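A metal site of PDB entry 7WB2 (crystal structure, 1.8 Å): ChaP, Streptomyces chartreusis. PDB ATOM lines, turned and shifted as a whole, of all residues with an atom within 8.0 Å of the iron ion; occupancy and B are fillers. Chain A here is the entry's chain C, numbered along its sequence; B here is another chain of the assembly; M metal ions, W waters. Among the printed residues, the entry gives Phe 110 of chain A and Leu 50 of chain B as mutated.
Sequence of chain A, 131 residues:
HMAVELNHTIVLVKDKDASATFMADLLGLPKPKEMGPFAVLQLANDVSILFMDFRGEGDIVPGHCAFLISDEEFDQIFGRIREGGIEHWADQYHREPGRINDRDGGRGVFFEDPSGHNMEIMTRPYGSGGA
The backbone NH (N) of Ala 66 lies within hydrogen-bond range of the backbone carbonyl oxygen (O) of His 8 of chain B, 2.9 Å away.
A ring nitrogen (ND1) of His 64 sits at hydrogen-bond distance from the backbone carbonyl oxygen (O) of Pro 62 (2.9 Å).
The backbone carbonyl oxygen (O) of His 64 is in hydrogen-bond range of the backbone NH (N) of Ile 10 of chain B (3.1 Å).
N of Glu 120 lies within hydrogen-bond range of O of Cys 65, 2.9 Å away.
The backbone carbonyl oxygen (O) of Glu 120 lies within hydrogen-bond range of the backbone NH (N) of Phe 67 (2.8 Å).
ND1 of His 8 of chain B sits at hydrogen-bond distance from OD1 of Asn 7 of chain B, 2.7 Å away.
Three residues have an atom within 4 Å of the iron ion: His 64, Glu 120 and His 8 of chain B.
The iron ion is bound by a ring nitrogen (NE2) of His 8 of chain B (2.1 Å), the side-chain carboxylate of Glu 120 (2.1 Å), a ring nitrogen (NE2) of His 64 (2.1 Å) and water W1 (2.4 Å).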
ATOM      1  N   PRO A  62      33.383 -20.642   8.340  1.00  0.00           N
ATOM      2  CA  PRO A  62      33.053 -19.374   7.671  1.00  0.00           C
ATOM      3  C   PRO A  62      32.235 -19.506   6.405  1.00  0.00           C
ATOM      4  O   PRO A  62      32.277 -18.581   5.573  1.00  0.00           O
ATOM      5  CB  PRO A  62      34.424 -18.809   7.359  1.00  0.00           C
ATOM      6  CG  PRO A  62      35.256 -20.055   7.050  1.00  0.00           C
ATOM      7  CD  PRO A  62      34.651 -21.190   7.845  1.00  0.00           C
ATOM      8  N   GLY A  63      31.512 -20.609   6.252  1.00  0.00           N
ATOM      9  CA  GLY A  63      30.600 -20.747   5.131  1.00  0.00           C
ATOM     10  C   GLY A  63      29.495 -19.702   5.178  1.00  0.00           C
ATOM     11  O   GLY A  63      29.092 -19.243   6.249  1.00  0.00           O
ATOM     12  N   HIS A  64      29.051 -19.268   4.000  1.00  0.00           N
ATOM     13  CA  HIS A  64      27.942 -18.325   3.911  1.00  0.00           C
ATOM     14  C   HIS A  64      27.479 -18.252   2.456  1.00  0.00           C
ATOM     15  O   HIS A  64      28.138 -18.758   1.546  1.00  0.00           O
ATOM     16  CB  HIS A  64      28.299 -16.934   4.432  1.00  0.00           C
ATOM     17  CG  HIS A  64      29.490 -16.315   3.769  1.00  0.00           C
ATOM     18  ND1 HIS A  64      30.795 -16.635   4.102  1.00  0.00           N
ATOM     19  CD2 HIS A  64      29.580 -15.348   2.828  1.00  0.00           C
ATOM     20  CE1 HIS A  64      31.622 -15.910   3.371  1.00  0.00           C
ATOM     21  NE2 HIS A  64      30.906 -15.119   2.598  1.00  0.00           N
ATOM     22  N   CYS A  65      26.292 -17.665   2.281  1.00  0.00           N
ATOM     23  CA  CYS A  65      25.808 -17.233   0.971  1.00  0.00           C
ATOM     24  C   CYS A  65      25.788 -15.716   0.963  1.00  0.00           C
ATOM     25  O   CYS A  65      25.295 -15.102   1.903  1.00  0.00           O
ATOM     26  CB  CYS A  65      24.416 -17.773   0.691  1.00  0.00           C
ATOM     27  SG  CYS A  65      24.368 -19.533   0.278  1.00  0.00           S
ATOM     28  N   ALA A  66      26.301 -15.114  -0.122  1.00  0.00           N
ATOM     29  CA  ALA A  66      26.569 -13.679  -0.160  1.00  0.00           C
ATOM     30  C   ALA A  66      25.781 -12.992  -1.258  1.00  0.00           C
ATOM     31  O   ALA A  66      25.772 -13.467  -2.397  1.00  0.00           O
ATOM     32  CB  ALA A  66      28.053 -13.414  -0.382  1.00  0.00           C
ATOM     33  N   PHE A  67      25.148 -11.874  -0.922  1.00  0.00           N
ATOM     34  CA  PHE A  67      24.334 -11.104  -1.843  1.00  0.00           C
ATOM     35  C   PHE A  67      24.951  -9.736  -2.052  1.00  0.00           C
ATOM     36  O   PHE A  67      25.336  -9.052  -1.096  1.00  0.00           O
ATOM     37  CB  PHE A  67      22.895 -10.999  -1.314  1.00  0.00           C
ATOM     38  CG  PHE A  67      22.249 -12.327  -1.098  1.00  0.00           C
ATOM     39  CD1 PHE A  67      21.575 -12.956  -2.129  1.00  0.00           C
ATOM     40  CD2 PHE A  67      22.395 -12.993   0.109  1.00  0.00           C
ATOM     41  CE1 PHE A  67      21.011 -14.216  -1.949  1.00  0.00           C
ATOM     42  CE2 PHE A  67      21.848 -14.246   0.305  1.00  0.00           C
ATOM     43  CZ  PHE A  67      21.153 -14.862  -0.729  1.00  0.00           C
ATOM     44  N   GLN A  92      33.181 -13.018   8.458  1.00  0.00           N
ATOM     45  CA  GLN A  92      32.632 -14.327   8.146  1.00  0.00           C
ATOM     46  C   GLN A  92      32.758 -15.330   9.284  1.00  0.00           C
ATOM     47  O   GLN A  92      32.051 -16.348   9.268  1.00  0.00           O
ATOM     48  CB  GLN A  92      33.323 -14.890   6.904  1.00  0.00           C
ATOM     49  CG  GLN A  92      34.829 -14.953   7.008  1.00  0.00           C
ATOM     50  CD  GLN A  92      35.463 -15.658   5.829  1.00  0.00           C
ATOM     51  OE1 GLN A  92      34.775 -16.062   4.891  1.00  0.00           O
ATOM     52  NE2 GLN A  92      36.782 -15.789   5.856  1.00  0.00           N
ATOM     53  N   PHE A 110      27.543  -9.710   7.989  1.00  0.00           N
ATOM     54  CA  PHE A 110      27.204 -11.126   8.002  1.00  0.00           C
ATOM     55  C   PHE A 110      26.114 -11.311   9.040  1.00  0.00           C
ATOM     56  O   PHE A 110      26.084 -10.617  10.058  1.00  0.00           O
ATOM     57  CB  PHE A 110      28.431 -11.995   8.344  1.00  0.00           C
ATOM     58  CG  PHE A 110      29.525 -11.922   7.314  1.00  0.00           C
ATOM     59  CD1 PHE A 110      30.421 -10.864   7.293  1.00  0.00           C
ATOM     60  CD2 PHE A 110      29.681 -12.950   6.383  1.00  0.00           C
ATOM     61  CE1 PHE A 110      31.418 -10.796   6.350  1.00  0.00           C
ATOM     62  CE2 PHE A 110      30.682 -12.885   5.431  1.00  0.00           C
ATOM     63  CZ  PHE A 110      31.556 -11.815   5.408  1.00  0.00           C
ATOM     64  N   MET A 119      24.622 -15.878   6.213  1.00  0.00           N
ATOM     65  CA  MET A 119      24.362 -14.970   5.098  1.00  0.00           C
ATOM     66  C   MET A 119      25.349 -13.807   5.112  1.00  0.00           C
ATOM     67  O   MET A 119      26.034 -13.550   6.114  1.00  0.00           O
ATOM     68  CB  MET A 119      22.927 -14.393   5.189  1.00  0.00           C
ATOM     69  CG  MET A 119      21.814 -15.440   5.124  1.00  0.00           C
ATOM     70  SD  MET A 119      21.838 -16.471   3.644  1.00  0.00           S
ATOM     71  CE  MET A 119      20.141 -17.023   3.536  1.00  0.00           C
ATOM     72  N   GLU A 120      25.431 -13.113   3.981  1.00  0.00           N
ATOM     73  CA  GLU A 120      26.271 -11.922   3.864  1.00  0.00           C
ATOM     74  C   GLU A 120      25.607 -10.995   2.857  1.00  0.00           C
ATOM     75  O   GLU A 120      25.104 -11.447   1.832  1.00  0.00           O
ATOM     76  CB  GLU A 120      27.706 -12.262   3.409  1.00  0.00           C
ATOM     77  CG  GLU A 120      28.626 -11.025   3.206  1.00  0.00           C
ATOM     78  CD  GLU A 120      29.950 -11.362   2.506  1.00  0.00           C
ATOM     79  OE1 GLU A 120      30.105 -12.505   2.089  1.00  0.00           O
ATOM     80  OE2 GLU A 120      30.823 -10.485   2.348  1.00  0.00           O
ATOM     81  N   ILE A 121      25.569  -9.701   3.187  1.00  0.00           N
ATOM     82  CA  ILE A 121      25.234  -8.682   2.194  1.00  0.00           C
ATOM     83  C   ILE A 121      26.426  -7.753   2.061  1.00  0.00           C
ATOM     84  O   ILE A 121      27.133  -7.488   3.035  1.00  0.00           O
ATOM     85  CB  ILE A 121      23.947  -7.922   2.557  1.00  0.00           C
ATOM     86  CG1 ILE A 121      24.079  -7.290   3.930  1.00  0.00           C
ATOM     87  CG2 ILE A 121      22.754  -8.861   2.509  1.00  0.00           C
ATOM     88  CD1 ILE A 121      23.017  -6.275   4.225  1.00  0.00           C
ATOM     89  N   MET A 122      26.641  -7.259   0.843  1.00  0.00           N
ATOM     90  CA  MET A 122      27.845  -6.495   0.523  1.00  0.00           C
ATOM     91  C   MET A 122      27.504  -5.512  -0.585  1.00  0.00           C
ATOM     92  O   MET A 122      26.647  -5.808  -1.417  1.00  0.00           O
ATOM     93  CB  MET A 122      28.970  -7.432   0.100  1.00  0.00           C
ATOM     94  CG  MET A 122      28.598  -8.283  -1.111  1.00  0.00           C
ATOM     95  SD  MET A 122      29.857  -9.484  -1.575  1.00  0.00           S
ATOM     96  CE  MET A 122      31.007  -8.489  -2.510  1.00  0.00           C
ATOM     97  N   ASN B   7      26.137 -13.151  -5.219  1.00  0.00           N
ATOM     98  CA  ASN B   7      27.513 -12.883  -5.626  1.00  0.00           C
ATOM     99  C   ASN B   7      28.466 -14.068  -5.411  1.00  0.00           C
ATOM    100  O   ASN B   7      29.365 -14.273  -6.226  1.00  0.00           O
ATOM    101  CB  ASN B   7      28.073 -11.667  -4.884  1.00  0.00           C
ATOM    102  CG  ASN B   7      29.471 -11.315  -5.347  1.00  0.00           C
ATOM    103  OD1 ASN B   7      30.455 -11.653  -4.709  1.00  0.00           O
ATOM    104  ND2 ASN B   7      29.570 -10.659  -6.491  1.00  0.00           N
ATOM    105  N   HIS B   8      28.330 -14.786  -4.306  1.00  0.00           N
ATOM    106  CA  HIS B   8      29.150 -15.985  -4.130  1.00  0.00           C
ATOM    107  C   HIS B   8      28.531 -16.883  -3.073  1.00  0.00           C
ATOM    108  O   HIS B   8      27.681 -16.447  -2.277  1.00  0.00           O
ATOM    109  CB  HIS B   8      30.615 -15.652  -3.765  1.00  0.00           C
ATOM    110  CG  HIS B   8      30.803 -14.784  -2.558  1.00  0.00           C
ATOM    111  ND1 HIS B   8      30.866 -13.403  -2.630  1.00  0.00           N
ATOM    112  CD2 HIS B   8      31.049 -15.090  -1.259  1.00  0.00           C
ATOM    113  CE1 HIS B   8      31.108 -12.904  -1.425  1.00  0.00           C
ATOM    114  NE2 HIS B   8      31.217 -13.903  -0.582  1.00  0.00           N
ATOM    115  N   THR B   9      28.922 -18.149  -3.092  1.00  0.00           N
ATOM    116  CA  THR B   9      28.461 -19.084  -2.079  1.00  0.00           C
ATOM    117  C   THR B   9      29.592 -20.040  -1.758  1.00  0.00           C
ATOM    118  O   THR B   9      30.382 -20.390  -2.634  1.00  0.00           O
ATOM    119  CB  THR B   9      27.190 -19.826  -2.520  1.00  0.00           C
ATOM    120  OG1 THR B   9      26.696 -20.628  -1.434  1.00  0.00           O
ATOM    121  CG2 THR B   9      27.471 -20.728  -3.709  1.00  0.00           C
ATOM    122  N   ILE B  10      29.708 -20.434  -0.493  1.00  0.00           N
ATOM    123  CA  ILE B  10      30.761 -21.341  -0.062  1.00  0.00           C
ATOM    124  C   ILE B  10      30.188 -22.746  -0.038  1.00  0.00           C
ATOM    125  O   ILE B  10      29.128 -22.990   0.541  1.00  0.00           O
ATOM    126  CB  ILE B  10      31.318 -20.943   1.328  1.00  0.00           C
ATOM    127  CG1 ILE B  10      32.258 -19.742   1.238  1.00  0.00           C
ATOM    128  CG2 ILE B  10      32.083 -22.139   1.984  1.00  0.00           C
ATOM    129  CD1 ILE B  10      31.540 -18.391   0.992  1.00  0.00           C
ATOM    130  N   MET B  35      42.296 -18.450  -2.083  1.00  0.00           N
ATOM    131  CA  MET B  35      42.081 -17.239  -1.292  1.00  0.00           C
ATOM    132  C   MET B  35      41.686 -17.665   0.123  1.00  0.00           C
ATOM    133  O   MET B  35      40.639 -18.291   0.321  1.00  0.00           O
ATOM    134  CB  MET B  35      41.051 -16.314  -1.949  1.00  0.00           C
ATOM    135  CG  MET B  35      39.616 -16.334  -1.430  1.00  0.00           C
ATOM    136  SD  MET B  35      38.701 -14.883  -1.980  1.00  0.00           S
ATOM    137  CE  MET B  35      39.157 -14.851  -3.717  1.00  0.00           C
ATOM    138  N   PHE B  38      39.828 -20.910   0.912  1.00  0.00           N
ATOM    139  CA  PHE B  38      38.900 -21.223  -0.174  1.00  0.00           C
ATOM    140  C   PHE B  38      39.633 -21.463  -1.495  1.00  0.00           C
ATOM    141  O   PHE B  38      40.651 -20.841  -1.796  1.00  0.00           O
ATOM    142  CB  PHE B  38      37.884 -20.088  -0.387  1.00  0.00           C
ATOM    143  CG  PHE B  38      37.084 -19.734   0.841  1.00  0.00           C
ATOM    144  CD1 PHE B  38      36.287 -20.667   1.467  1.00  0.00           C
ATOM    145  CD2 PHE B  38      37.095 -18.425   1.336  1.00  0.00           C
ATOM    146  CE1 PHE B  38      35.532 -20.336   2.595  1.00  0.00           C
ATOM    147  CE2 PHE B  38      36.347 -18.084   2.453  1.00  0.00           C
ATOM    148  CZ  PHE B  38      35.564 -19.040   3.093  1.00  0.00           C
ATOM    149  N   LEU B  50      32.943 -20.854  -3.745  1.00  0.00           N
ATOM    150  CA  LEU B  50      34.135 -20.887  -2.913  1.00  0.00           C
ATOM    151  C   LEU B  50      34.159 -22.250  -2.224  1.00  0.00           C
ATOM    152  O   LEU B  50      33.409 -22.477  -1.265  1.00  0.00           O
ATOM    153  CB  LEU B  50      34.155 -19.736  -1.918  1.00  0.00           C
ATOM    154  CG  LEU B  50      34.674 -18.394  -2.493  1.00  0.00           C
ATOM    155  CD1 LEU B  50      33.664 -17.792  -3.447  1.00  0.00           C
ATOM    156  CD2 LEU B  50      35.020 -17.412  -1.387  1.00  0.00           C
HETATM  157 FE    FE M   1      31.721 -13.616   1.401  1.00  0.00          FE
HETATM  158  O   HOH W   1      33.857 -14.557   1.043  1.00  0.00           O
